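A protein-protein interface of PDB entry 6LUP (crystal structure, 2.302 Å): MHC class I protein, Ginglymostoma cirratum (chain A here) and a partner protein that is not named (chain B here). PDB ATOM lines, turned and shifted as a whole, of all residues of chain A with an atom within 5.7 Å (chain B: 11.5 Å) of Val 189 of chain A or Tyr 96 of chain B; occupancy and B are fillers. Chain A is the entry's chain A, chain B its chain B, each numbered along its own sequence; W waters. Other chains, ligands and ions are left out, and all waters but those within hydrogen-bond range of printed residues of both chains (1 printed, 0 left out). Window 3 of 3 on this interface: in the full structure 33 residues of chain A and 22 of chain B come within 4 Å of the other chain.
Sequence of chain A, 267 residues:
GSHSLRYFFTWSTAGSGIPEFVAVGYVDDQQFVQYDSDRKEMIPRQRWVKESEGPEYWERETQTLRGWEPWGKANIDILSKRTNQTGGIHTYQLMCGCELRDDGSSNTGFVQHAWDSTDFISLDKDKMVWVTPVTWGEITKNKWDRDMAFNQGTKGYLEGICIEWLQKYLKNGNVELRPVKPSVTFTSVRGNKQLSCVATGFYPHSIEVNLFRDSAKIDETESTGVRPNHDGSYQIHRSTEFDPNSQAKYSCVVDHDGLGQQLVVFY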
ATOM      1  N   THR A 187       0.432  -5.051  33.161  1.00  0.00           N
ATOM      2  CA  THR A 187       0.646  -3.700  33.677  1.00  0.00           C
ATOM      3  C   THR A 187      -0.175  -3.414  34.929  1.00  0.00           C
ATOM      4  O   THR A 187      -1.212  -4.044  35.167  1.00  0.00           O
ATOM      5  CB  THR A 187       0.276  -2.629  32.627  1.00  0.00           C
ATOM      6  OG1 THR A 187      -1.045  -2.878  32.131  1.00  0.00           O
ATOM      7  CG2 THR A 187       1.265  -2.621  31.467  1.00  0.00           C
ATOM      8  N   SER A 188       0.297  -2.453  35.723  1.00  0.00           N
ATOM      9  CA  SER A 188      -0.483  -1.916  36.829  1.00  0.00           C
ATOM     10  C   SER A 188      -1.606  -1.070  36.254  1.00  0.00           C
ATOM     11  O   SER A 188      -1.407  -0.338  35.280  1.00  0.00           O
ATOM     12  CB  SER A 188       0.392  -1.075  37.765  1.00  0.00           C
ATOM     13  OG  SER A 188       0.741   0.167  37.173  1.00  0.00           O
ATOM     14  N   VAL A 189      -2.787  -1.177  36.856  1.00  0.00           N
ATOM     15  CA  VAL A 189      -3.977  -0.492  36.352  1.00  0.00           C
ATOM     16  C   VAL A 189      -4.900  -0.051  37.498  1.00  0.00           C
ATOM     17  O   VAL A 189      -4.670  -0.413  38.657  1.00  0.00           O
ATOM     18  CB  VAL A 189      -4.754  -1.372  35.336  1.00  0.00           C
ATOM     19  CG1 VAL A 189      -3.978  -1.546  34.029  1.00  0.00           C
ATOM     20  CG2 VAL A 189      -5.117  -2.718  35.948  1.00  0.00           C
ATOM     21  N   ARG A 190      -5.931   0.730  37.164  1.00  0.00           N
ATOM     22  CA  ARG A 190      -6.900   1.277  38.135  1.00  0.00           C
ATOM     23  C   ARG A 190      -6.237   2.099  39.247  1.00  0.00           C
ATOM     24  O   ARG A 190      -6.618   2.002  40.419  1.00  0.00           O
ATOM     25  CB  ARG A 190      -7.778   0.173  38.745  1.00  0.00           C
ATOM     26  CG  ARG A 190      -8.634  -0.592  37.752  1.00  0.00           C
ATOM     27  CD  ARG A 190      -9.512  -1.600  38.474  1.00  0.00           C
ATOM     28  NE  ARG A 190     -10.065  -2.609  37.568  1.00  0.00           N
ATOM     29  CZ  ARG A 190     -11.186  -2.463  36.865  1.00  0.00           C
ATOM     30  NH1 ARG A 190     -11.601  -3.446  36.075  1.00  0.00           N
ATOM     31  NH2 ARG A 190     -11.897  -1.344  36.947  1.00  0.00           N
ATOM     32  N   GLY A 191      -5.251   2.906  38.866  1.00  0.00           N
ATOM     33  CA  GLY A 191      -4.483   3.702  39.819  1.00  0.00           C
ATOM     34  C   GLY A 191      -3.593   2.844  40.700  1.00  0.00           C
ATOM     35  O   GLY A 191      -3.572   3.012  41.920  1.00  0.00           O
ATOM     36  N   ASN A 192      -2.874   1.914  40.071  1.00  0.00           N
ATOM     37  CA  ASN A 192      -1.933   1.011  40.751  1.00  0.00           C
ATOM     38  C   ASN A 192      -2.551   0.132  41.851  1.00  0.00           C
ATOM     39  O   ASN A 192      -1.837  -0.491  42.642  1.00  0.00           O
ATOM     40  CB  ASN A 192      -0.712   1.782  41.276  1.00  0.00           C
ATOM     41  CG  ASN A 192       0.136   2.362  40.160  1.00  0.00           C
ATOM     42  OD1 ASN A 192       1.227   1.868  39.880  1.00  0.00           O
ATOM     43  ND2 ASN A 192      -0.364   3.412  39.510  1.00  0.00           N
ATOM     44  N   LYS A 193      -3.880   0.084  41.873  1.00  0.00           N
ATOM     45  CA  LYS A 193      -4.635  -0.749  42.805  1.00  0.00           C
ATOM     46  C   LYS A 193      -4.561  -2.228  42.408  1.00  0.00           C
ATOM     47  O   LYS A 193      -4.435  -3.100  43.269  1.00  0.00           O
ATOM     48  CB  LYS A 193      -6.094  -0.267  42.873  1.00  0.00           C
ATOM     49  CG  LYS A 193      -7.013  -1.057  43.796  1.00  0.00           C
ATOM     50  CD  LYS A 193      -8.330  -0.324  44.017  1.00  0.00           C
ATOM     51  CE  LYS A 193      -9.403  -1.233  44.612  1.00  0.00           C
ATOM     52  NZ  LYS A 193     -10.063  -2.099  43.590  1.00  0.00           N
ATOM     53  N   GLN A 194      -4.637  -2.502  41.106  1.00  0.00           N
ATOM     54  CA  GLN A 194      -4.663  -3.877  40.605  1.00  0.00           C
ATOM     55  C   GLN A 194      -3.634  -4.126  39.506  1.00  0.00           C
ATOM     56  O   GLN A 194      -3.232  -3.204  38.791  1.00  0.00           O
ATOM     57  CB  GLN A 194      -6.066  -4.249  40.113  1.00  0.00           C
ATOM     58  CG  GLN A 194      -7.161  -4.000  41.137  1.00  0.00           C
ATOM     59  CD  GLN A 194      -8.369  -4.892  40.949  1.00  0.00           C
ATOM     60  OE1 GLN A 194      -8.241  -6.097  40.725  1.00  0.00           O
ATOM     61  NE2 GLN A 194      -9.557  -4.307  41.058  1.00  0.00           N
ATOM     62  N   LEU A 195      -3.206  -5.379  39.391  1.00  0.00           N
ATOM     63  CA  LEU A 195      -2.263  -5.786  38.359  1.00  0.00           C
ATOM     64  C   LEU A 195      -2.980  -6.705  37.380  1.00  0.00           C
ATOM     65  O   LEU A 195      -3.482  -7.759  37.771  1.00  0.00           O
ATOM     66  CB  LEU A 195      -1.067  -6.496  38.992  1.00  0.00           C
ATOM     67  CG  LEU A 195       0.295  -6.343  38.309  1.00  0.00           C
ATOM     68  CD1 LEU A 195       0.828  -4.924  38.456  1.00  0.00           C
ATOM     69  CD2 LEU A 195       1.282  -7.337  38.901  1.00  0.00           C
ATOM     70  N   SER A 196      -3.036  -6.304  36.111  1.00  0.00           N
ATOM     71  CA  SER A 196      -3.868  -7.007  35.136  1.00  0.00           C
ATOM     72  C   SER A 196      -3.105  -7.598  33.959  1.00  0.00           C
ATOM     73  O   SER A 196      -2.375  -6.900  33.250  1.00  0.00           O
ATOM     74  CB  SER A 196      -4.987  -6.100  34.626  1.00  0.00           C
ATOM     75  OG  SER A 196      -5.987  -6.854  33.963  1.00  0.00           O
ATOM     76  N   VAL A 198      -3.618  -9.053  30.417  1.00  0.00           N
ATOM     77  CA  VAL A 198      -4.572  -9.045  29.311  1.00  0.00           C
ATOM     78  C   VAL A 198      -3.984  -9.660  28.039  1.00  0.00           C
ATOM     79  O   VAL A 198      -2.985  -9.176  27.497  1.00  0.00           O
ATOM     80  CB  VAL A 198      -5.172  -7.632  29.058  1.00  0.00           C
ATOM     81  CG1 VAL A 198      -4.114  -6.544  29.166  1.00  0.00           C
ATOM     82  CG2 VAL A 198      -5.894  -7.570  27.714  1.00  0.00           C
ATOM     83  N   THR A 224     -12.269 -12.018  33.565  1.00  0.00           N
ATOM     84  CA  THR A 224     -13.418 -11.775  32.699  1.00  0.00           C
ATOM     85  C   THR A 224     -13.873 -13.070  32.040  1.00  0.00           C
ATOM     86  O   THR A 224     -15.040 -13.212  31.683  1.00  0.00           O
ATOM     87  CB  THR A 224     -13.096 -10.771  31.570  1.00  0.00           C
ATOM     88  OG1 THR A 224     -11.993 -11.249  30.785  1.00  0.00           O
ATOM     89  CG2 THR A 224     -12.787  -9.392  32.131  1.00  0.00           C
ATOM     90  N   HIS A 237      -9.000 -11.045  30.334  1.00  0.00           N
ATOM     91  CA  HIS A 237      -8.338 -10.247  31.356  1.00  0.00           C
ATOM     92  C   HIS A 237      -8.316 -11.041  32.650  1.00  0.00           C
ATOM     93  O   HIS A 237      -9.368 -11.441  33.150  1.00  0.00           O
ATOM     94  CB  HIS A 237      -9.084  -8.929  31.585  1.00  0.00           C
ATOM     95  CG  HIS A 237      -9.054  -7.994  30.415  1.00  0.00           C
ATOM     96  ND1 HIS A 237      -8.511  -6.730  30.490  1.00  0.00           N
ATOM     97  CD2 HIS A 237      -9.508  -8.133  29.147  1.00  0.00           C
ATOM     98  CE1 HIS A 237      -8.632  -6.129  29.319  1.00  0.00           C
ATOM     99  NE2 HIS A 237      -9.231  -6.961  28.486  1.00  0.00           N
ATOM    100  N   SER A 239      -6.851 -10.383  36.488  1.00  0.00           N
ATOM    101  CA  SER A 239      -6.274  -9.382  37.380  1.00  0.00           C
ATOM    102  C   SER A 239      -6.332  -9.795  38.846  1.00  0.00           C
ATOM    103  O   SER A 239      -7.256 -10.492  39.282  1.00  0.00           O
ATOM    104  CB  SER A 239      -6.968  -8.032  37.192  1.00  0.00           C
ATOM    105  OG  SER A 239      -8.362  -8.152  37.409  1.00  0.00           O
ATOM    106  N   GLN B   8     -21.045  -8.025  29.005  1.00  0.00           N
ATOM    107  CA  GLN B   8     -19.780  -7.319  29.174  1.00  0.00           C
ATOM    108  C   GLN B   8     -19.623  -6.258  28.095  1.00  0.00           C
ATOM    109  O   GLN B   8     -20.007  -6.473  26.945  1.00  0.00           O
ATOM    110  CB  GLN B   8     -18.606  -8.293  29.119  1.00  0.00           C
ATOM    111  CG  GLN B   8     -18.499  -9.199  30.327  1.00  0.00           C
ATOM    112  CD  GLN B   8     -17.444 -10.264  30.157  1.00  0.00           C
ATOM    113  OE1 GLN B   8     -17.681 -11.298  29.536  1.00  0.00           O
ATOM    114  NE2 GLN B   8     -16.272 -10.025  30.718  1.00  0.00           N
ATOM    115  N   VAL B   9     -19.075  -5.105  28.464  1.00  0.00           N
ATOM    116  CA  VAL B   9     -18.719  -4.096  27.470  1.00  0.00           C
ATOM    117  C   VAL B   9     -17.254  -3.717  27.620  1.00  0.00           C
ATOM    118  O   VAL B   9     -16.792  -3.393  28.716  1.00  0.00           O
ATOM    119  CB  VAL B   9     -19.642  -2.853  27.487  1.00  0.00           C
ATOM    120  CG1 VAL B   9     -21.096  -3.258  27.332  1.00  0.00           C
ATOM    121  CG2 VAL B   9     -19.476  -2.072  28.768  1.00  0.00           C
ATOM    122  N   TYR B  10     -16.527  -3.775  26.511  1.00  0.00           N
ATOM    123  CA  TYR B  10     -15.077  -3.672  26.535  1.00  0.00           C
ATOM    124  C   TYR B  10     -14.543  -3.252  25.177  1.00  0.00           C
ATOM    125  O   TYR B  10     -15.302  -3.124  24.218  1.00  0.00           O
ATOM    126  CB  TYR B  10     -14.472  -5.015  26.943  1.00  0.00           C
ATOM    127  CG  TYR B  10     -14.981  -6.191  26.134  1.00  0.00           C
ATOM    128  CD1 TYR B  10     -16.213  -6.783  26.424  1.00  0.00           C
ATOM    129  CD2 TYR B  10     -14.227  -6.715  25.083  1.00  0.00           C
ATOM    130  CE1 TYR B  10     -16.682  -7.854  25.689  1.00  0.00           C
ATOM    131  CE2 TYR B  10     -14.687  -7.790  24.344  1.00  0.00           C
ATOM    132  CZ  TYR B  10     -15.915  -8.352  24.651  1.00  0.00           C
ATOM    133  OH  TYR B  10     -16.375  -9.422  23.921  1.00  0.00           O
ATOM    134  N   THR B  11     -13.233  -3.035  25.106  1.00  0.00           N
ATOM    135  CA  THR B  11     -12.577  -2.654  23.862  1.00  0.00           C
ATOM    136  C   THR B  11     -11.588  -3.722  23.422  1.00  0.00           C
ATOM    137  O   THR B  11     -11.164  -4.551  24.224  1.00  0.00           O
ATOM    138  CB  THR B  11     -11.858  -1.294  23.980  1.00  0.00           C
ATOM    139  OG1 THR B  11     -10.838  -1.372  24.980  1.00  0.00           O
ATOM    140  CG2 THR B  11     -12.844  -0.198  24.337  1.00  0.00           C
ATOM    141  N   TYR B  12     -11.226  -3.694  22.143  1.00  0.00           N
ATOM    142  CA  TYR B  12     -10.343  -4.697  21.552  1.00  0.00           C
ATOM    143  C   TYR B  12      -8.939  -4.635  22.141  1.00  0.00           C
ATOM    144  O   TYR B  12      -8.341  -5.663  22.465  1.00  0.00           O
ATOM    145  CB  TYR B  12     -10.300  -4.529  20.025  1.00  0.00           C
ATOM    146  CG  TYR B  12      -9.174  -5.272  19.342  1.00  0.00           C
ATOM    147  CD1 TYR B  12      -9.156  -6.666  19.302  1.00  0.00           C
ATOM    148  CD2 TYR B  12      -8.130  -4.580  18.727  1.00  0.00           C
ATOM    149  CE1 TYR B  12      -8.126  -7.350  18.677  1.00  0.00           C
ATOM    150  CE2 TYR B  12      -7.093  -5.257  18.098  1.00  0.00           C
ATOM    151  CZ  TYR B  12      -7.099  -6.642  18.076  1.00  0.00           C
ATOM    152  OH  TYR B  12      -6.078  -7.319  17.458  1.00  0.00           O
ATOM    153  N   LYS B  13      -8.433  -3.417  22.274  1.00  0.00           N
ATOM    154  CA  LYS B  13      -7.082  -3.165  22.734  1.00  0.00           C
ATOM    155  C   LYS B  13      -7.191  -2.240  23.948  1.00  0.00           C
ATOM    156  O   LYS B  13      -8.295  -1.843  24.328  1.00  0.00           O
ATOM    157  CB  LYS B  13      -6.294  -2.502  21.597  1.00  0.00           C
ATOM    158  CG  LYS B  13      -4.780  -2.604  21.678  1.00  0.00           C
ATOM    159  CD  LYS B  13      -4.136  -1.860  20.515  1.00  0.00           C
ATOM    160  CE  LYS B  13      -2.695  -1.478  20.817  1.00  0.00           C
ATOM    161  NZ  LYS B  13      -2.139  -0.557  19.785  1.00  0.00           N
ATOM    162  N   LEU B  14      -6.057  -1.912  24.564  1.00  0.00           N
ATOM    163  CA  LEU B  14      -6.030  -0.938  25.651  1.00  0.00           C
ATOM    164  C   LEU B  14      -6.361   0.459  25.125  1.00  0.00           C
ATOM    165  O   LEU B  14      -5.749   0.924  24.159  1.00  0.00           O
ATOM    166  CB  LEU B  14      -4.663  -0.939  26.347  1.00  0.00           C
ATOM    167  CG  LEU B  14      -4.441   0.058  27.495  1.00  0.00           C
ATOM    168  CD1 LEU B  14      -5.140  -0.396  28.771  1.00  0.00           C
ATOM    169  CD2 LEU B  14      -2.953   0.277  27.740  1.00  0.00           C
ATOM    170  N   ILE B  15      -7.332   1.109  25.764  1.00  0.00           N
ATOM    171  CA  ILE B  15      -7.781   2.447  25.371  1.00  0.00           C
ATOM    172  C   ILE B  15      -6.672   3.488  25.501  1.00  0.00           C
ATOM    173  O   ILE B  15      -6.026   3.597  26.544  1.00  0.00           O
ATOM    174  CB  ILE B  15      -9.006   2.910  26.195  1.00  0.00           C
ATOM    175  CG1 ILE B  15     -10.222   2.027  25.901  1.00  0.00           C
ATOM    176  CG2 ILE B  15      -9.333   4.374  25.908  1.00  0.00           C
ATOM    177  CD1 ILE B  15     -11.377   2.209  26.866  1.00  0.00           C
ATOM    178  N   LYS B  16      -6.452   4.224  24.415  1.00  0.00           N
ATOM    179  CA  LYS B  16      -5.632   5.431  24.404  1.00  0.00           C
ATOM    180  C   LYS B  16      -6.457   6.503  23.707  1.00  0.00           C
ATOM    181  O   LYS B  16      -7.004   6.264  22.630  1.00  0.00           O
ATOM    182  CB  LYS B  16      -4.328   5.212  23.633  1.00  0.00           C
ATOM    183  CG  LYS B  16      -3.382   4.172  24.220  1.00  0.00           C
ATOM    184  CD  LYS B  16      -2.188   3.929  23.304  1.00  0.00           C
ATOM    185  CE  LYS B  16      -1.239   5.120  23.279  1.00  0.00           C
ATOM    186  NZ  LYS B  16      -0.174   4.958  22.252  1.00  0.00           N
ATOM    187  N   GLU B  17      -6.560   7.679  24.319  1.00  0.00           N
ATOM    188  CA  GLU B  17      -7.352   8.766  23.748  1.00  0.00           C
ATOM    189  C   GLU B  17      -6.776   9.183  22.394  1.00  0.00           C
ATOM    190  O   GLU B  17      -5.584   9.472  22.283  1.00  0.00           O
ATOM    191  CB  GLU B  17      -7.431   9.965  24.705  1.00  0.00           C
ATOM    192  CG  GLU B  17      -7.558   9.624  26.192  1.00  0.00           C
ATOM    193  CD  GLU B  17      -8.836   8.876  26.563  1.00  0.00           C
ATOM    194  OE1 GLU B  17      -8.918   8.392  27.711  1.00  0.00           O
ATOM    195  OE2 GLU B  17      -9.762   8.770  25.727  1.00  0.00           O
ATOM    196  N   ASN B  21      -9.877   2.356  18.163  1.00  0.00           N
ATOM    197  CA  ASN B  21     -10.119   1.053  18.780  1.00  0.00           C
ATOM    198  C   ASN B  21     -11.461   0.455  18.321  1.00  0.00           C
ATOM    199  O   ASN B  21     -12.148   1.027  17.467  1.00  0.00           O
ATOM    200  CB  ASN B  21     -10.086   1.193  20.310  1.00  0.00           C
ATOM    201  CG  ASN B  21      -9.564  -0.053  21.012  1.00  0.00           C
ATOM    202  OD1 ASN B  21     -10.128  -1.142  20.886  1.00  0.00           O
ATOM    203  ND2 ASN B  21      -8.488   0.111  21.773  1.00  0.00           N
ATOM    204  N   PHE B  70     -14.247   2.586  16.487  1.00  0.00           N
ATOM    205  CA  PHE B  70     -14.468   3.900  17.099  1.00  0.00           C
ATOM    206  C   PHE B  70     -13.179   4.577  17.556  1.00  0.00           C
ATOM    207  O   PHE B  70     -12.125   3.938  17.648  1.00  0.00           O
ATOM    208  CB  PHE B  70     -15.475   3.798  18.264  1.00  0.00           C
ATOM    209  CG  PHE B  70     -14.861   3.432  19.596  1.00  0.00           C
ATOM    210  CD1 PHE B  70     -14.123   2.260  19.754  1.00  0.00           C
ATOM    211  CD2 PHE B  70     -15.049   4.251  20.705  1.00  0.00           C
ATOM    212  CE1 PHE B  70     -13.569   1.927  20.980  1.00  0.00           C
ATOM    213  CE2 PHE B  70     -14.504   3.920  21.936  1.00  0.00           C
ATOM    214  CZ  PHE B  70     -13.761   2.757  22.073  1.00  0.00           C
ATOM    215  N   PRO B  72     -12.112   6.614  20.924  1.00  0.00           N
ATOM    216  CA  PRO B  72     -12.403   7.154  22.251  1.00  0.00           C
ATOM    217  C   PRO B  72     -11.802   8.547  22.440  1.00  0.00           C
ATOM    218  O   PRO B  72     -10.592   8.735  22.291  1.00  0.00           O
ATOM    219  CB  PRO B  72     -11.757   6.139  23.201  1.00  0.00           C
ATOM    220  CG  PRO B  72     -10.744   5.417  22.384  1.00  0.00           C
ATOM    221  CD  PRO B  72     -11.284   5.394  20.986  1.00  0.00           C
ATOM    222  N   SER B  74     -11.311  12.048  24.953  1.00  0.00           N
ATOM    223  CA  SER B  74     -11.004  12.291  26.366  1.00  0.00           C
ATOM    224  C   SER B  74     -12.237  12.316  27.268  1.00  0.00           C
ATOM    225  O   SER B  74     -12.295  11.596  28.264  1.00  0.00           O
ATOM    226  CB  SER B  74     -10.214  13.592  26.522  1.00  0.00           C
ATOM    227  OG  SER B  74      -9.010  13.547  25.775  1.00  0.00           O
ATOM    228  N   TYR B  76     -15.570  11.570  26.548  1.00  0.00           N
ATOM    229  CA  TYR B  76     -16.734  10.723  26.236  1.00  0.00           C
ATOM    230  C   TYR B  76     -16.958   9.472  27.098  1.00  0.00           C
ATOM    231  O   TYR B  76     -16.012   8.765  27.453  1.00  0.00           O
ATOM    232  CB  TYR B  76     -16.746  10.352  24.746  1.00  0.00           C
ATOM    233  CG  TYR B  76     -17.229  11.467  23.838  1.00  0.00           C
ATOM    234  CD1 TYR B  76     -18.488  12.033  24.009  1.00  0.00           C
ATOM    235  CD2 TYR B  76     -16.434  11.946  22.802  1.00  0.00           C
ATOM    236  CE1 TYR B  76     -18.938  13.053  23.181  1.00  0.00           C
ATOM    237  CE2 TYR B  76     -16.874  12.965  21.967  1.00  0.00           C
ATOM    238  CZ  TYR B  76     -18.128  13.513  22.163  1.00  0.00           C
ATOM    239  OH  TYR B  76     -18.578  14.523  21.345  1.00  0.00           O
ATOM    240  N   TYR B  78     -19.089   5.763  27.491  1.00  0.00           N
ATOM    241  CA  TYR B  78     -19.625   4.704  26.635  1.00  0.00           C
ATOM    242  C   TYR B  78     -20.390   3.649  27.419  1.00  0.00           C
ATOM    243  O   TYR B  78     -20.035   3.331  28.554  1.00  0.00           O
ATOM    244  CB  TYR B  78     -18.497   4.041  25.842  1.00  0.00           C
ATOM    245  CG  TYR B  78     -17.679   5.010  25.020  1.00  0.00           C
ATOM    246  CD1 TYR B  78     -18.045   5.327  23.710  1.00  0.00           C
ATOM    247  CD2 TYR B  78     -16.546   5.622  25.553  1.00  0.00           C
ATOM    248  CE1 TYR B  78     -17.300   6.220  22.957  1.00  0.00           C
ATOM    249  CE2 TYR B  78     -15.796   6.517  24.806  1.00  0.00           C
ATOM    250  CZ  TYR B  78     -16.177   6.811  23.511  1.00  0.00           C
ATOM    251  OH  TYR B  78     -15.433   7.697  22.771  1.00  0.00           O
ATOM    252  N   GLN B  92     -22.263   0.113  31.714  1.00  0.00           N
ATOM    253  CA  GLN B  92     -21.213   1.079  31.400  1.00  0.00           C
ATOM    254  C   GLN B  92     -19.895   0.418  31.021  1.00  0.00           C
ATOM    255  O   GLN B  92     -19.582  -0.676  31.491  1.00  0.00           O
ATOM    256  CB  GLN B  92     -20.985   2.028  32.580  1.00  0.00           C
ATOM    257  CG  GLN B  92     -21.253   3.497  32.274  1.00  0.00           C
ATOM    258  CD  GLN B  92     -22.694   3.789  31.895  1.00  0.00           C
ATOM    259  OE1 GLN B  92     -23.630   3.169  32.405  1.00  0.00           O
ATOM    260  NE2 GLN B  92     -22.876   4.744  31.000  1.00  0.00           N
ATOM    261  N   LEU B  93     -19.128   1.097  30.169  1.00  0.00           N
ATOM    262  CA  LEU B  93     -17.768   0.681  29.843  1.00  0.00           C
ATOM    263  C   LEU B  93     -16.871   0.832  31.064  1.00  0.00           C
ATOM    264  O   LEU B  93     -16.661   1.940  31.563  1.00  0.00           O
ATOM    265  CB  LEU B  93     -17.211   1.480  28.654  1.00  0.00           C
ATOM    266  CG  LEU B  93     -15.717   1.355  28.313  1.00  0.00           C
ATOM    267  CD1 LEU B  93     -15.376   0.007  27.693  1.00  0.00           C
ATOM    268  CD2 LEU B  93     -15.284   2.484  27.394  1.00  0.00           C
ATOM    269  N   ASP B  94     -16.358  -0.296  31.545  1.00  0.00           N
ATOM    270  CA  ASP B  94     -15.407  -0.306  32.645  1.00  0.00           C
ATOM    271  C   ASP B  94     -14.015  -0.002  32.103  1.00  0.00           C
ATOM    272  O   ASP B  94     -13.498  -0.737  31.255  1.00  0.00           O
ATOM    273  CB  ASP B  94     -15.425  -1.667  33.347  1.00  0.00           C
ATOM    274  CG  ASP B  94     -14.729  -1.646  34.701  1.00  0.00           C
ATOM    275  OD1 ASP B  94     -14.119  -0.615  35.066  1.00  0.00           O
ATOM    276  OD2 ASP B  94     -14.794  -2.676  35.404  1.00  0.00           O
ATOM    277  N   ARG B  95     -13.418   1.083  32.587  1.00  0.00           N
ATOM    278  CA  ARG B  95     -12.087   1.477  32.131  1.00  0.00           C
ATOM    279  C   ARG B  95     -10.998   1.169  33.162  1.00  0.00           C
ATOM    280  O   ARG B  95     -11.266   1.050  34.361  1.00  0.00           O
ATOM    281  CB  ARG B  95     -12.050   2.951  31.707  1.00  0.00           C
ATOM    282  CG  ARG B  95     -11.016   3.230  30.624  1.00  0.00           C
ATOM    283  CD  ARG B  95     -11.015   4.678  30.165  1.00  0.00           C
ATOM    284  NE  ARG B  95     -12.238   5.039  29.453  1.00  0.00           N
ATOM    285  CZ  ARG B  95     -12.376   6.120  28.689  1.00  0.00           C
ATOM    286  NH1 ARG B  95     -11.363   6.961  28.518  1.00  0.00           N
ATOM    287  NH2 ARG B  95     -13.532   6.361  28.089  1.00  0.00           N
ATOM    288  N   TYR B  96      -9.770   1.037  32.663  1.00  0.00           N
ATOM    289  CA  TYR B  96      -8.609   0.658  33.461  1.00  0.00           C
ATOM    290  C   TYR B  96      -7.815   1.873  33.934  1.00  0.00           C
ATOM    291  O   TYR B  96      -8.382   2.929  34.214  1.00  0.00           O
ATOM    292  CB  TYR B  96      -7.707  -0.275  32.643  1.00  0.00           C
ATOM    293  CG  TYR B  96      -8.023  -1.757  32.771  1.00  0.00           C
ATOM    294  CD1 TYR B  96      -9.172  -2.202  33.435  1.00  0.00           C
ATOM    295  CD2 TYR B  96      -7.180  -2.715  32.207  1.00  0.00           C
ATOM    296  CE1 TYR B  96      -9.456  -3.554  33.547  1.00  0.00           C
ATOM    297  CE2 TYR B  96      -7.459  -4.071  32.313  1.00  0.00           C
ATOM    298  CZ  TYR B  96      -8.596  -4.484  32.983  1.00  0.00           C
ATOM    299  OH  TYR B  96      -8.880  -5.826  33.091  1.00  0.00           O
HETATM  300  O   HOH W   1     -16.287 -13.936  29.213  1.00  0.00           O
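The side-chain hydroxyl (OG) of Ser 196 of chain A sits at hydrogen-bond distance from the side-chain hydroxyl (OH) of Tyr 96 of chain B (3.2 Å). NH2 of Arg 190 of chain A is in salt-bridge range of OD1 of Asp 94 of chain B. ND1 of His 237 of chain A is in hydrogen-bond range of OH of Tyr 96 of chain B, 2.8 Å away.
OE1 of Glu 17 of chain B is in salt-bridge range of NH1 of Arg 95 of chain B (2.9 Å). The backbone NH (N) of Ser 196 of chain A sits at hydrogen-bond distance from the backbone carbonyl oxygen (O) of Thr 187 of chain A (3.1 Å). The backbone NH of Thr 224 of chain A sits at hydrogen-bond distance from the backbone carbonyl oxygen of His 237 of chain A (3.0 Å). The backbone carbonyl oxygen (O) of Gln 194 of chain A lies within hydrogen-bond range of the backbone NH (N) of Val 189 of chain A, 2.8 Å away.
Among the printed residues, pairs that only touch across the chains: Arg 190 of chain A with Tyr 96 of chain B, Thr 224 of chain A with Gln 8 of chain B, Arg 190 of chain A with Arg 95 of chain B and Val 189 of chain A with Tyr 96 of chain B.
No residue of chain B comes within 4 Å of Thr 187 of chain A. Val 189 of chain A touches just one residue of chain B: Tyr 96 (3.9 Å). Of chain B, only Asp 94 (3.0 Å), Arg 95 (3.6 Å) and Tyr 96 (3.3 Å) come within 4 Å of Arg 190 of chain A. No residue of chain B comes within 4 Å of Gly 191 of chain A. Gln 194 of chain A touches none of the printed residues of chain B. Ser 196 of chain A touches one residue of chain B. Of the printed residues of chain B, Thr 224 of chain A touches Gln 8 (3.4 Å). Printed residues of chain A within 4 Å of Gln 8 of chain B: Thr 224. Leu 14 of chain B touches none of the printed residues of chain A. Ser 74 of chain B touches none of the printed residues of chain A. Printed residues of chain A within 4 Å of Asp 94 of chain B: Arg 190. Printed residues of chain A within 4 Å of Arg 95 of chain B: Arg 190. Tyr 96 of chain B touches four residues of chain A. The nearest residue of chain A that does not touch Tyr 96 of chain B is Ser 239 of chain A (4.9 Å).
Printed residues of chain A that touch a printed residue of chain B: Val 189, Arg 190, Ser 196, Thr 224 and His 237. Along chain A the printed residues that touch a printed residue of chain B span positions 189 to 237. Printed residues of chain B that touch a printed residue of chain A: Gln 8, Asp 94, Arg 95 and Tyr 96. Among the printed residues, Asp or Glu carboxylates within 4 Å of a Lys or Arg side-chain nitrogen of the other chain: Arg 190 of chain A with Asp 94 of chain B.
Water W1 bridges the backbone carbonyl oxygen of Thr 224 of chain A (2.9 Å) and the side-chain amide oxygen of Gln 8 of chain B (3.0 Å).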
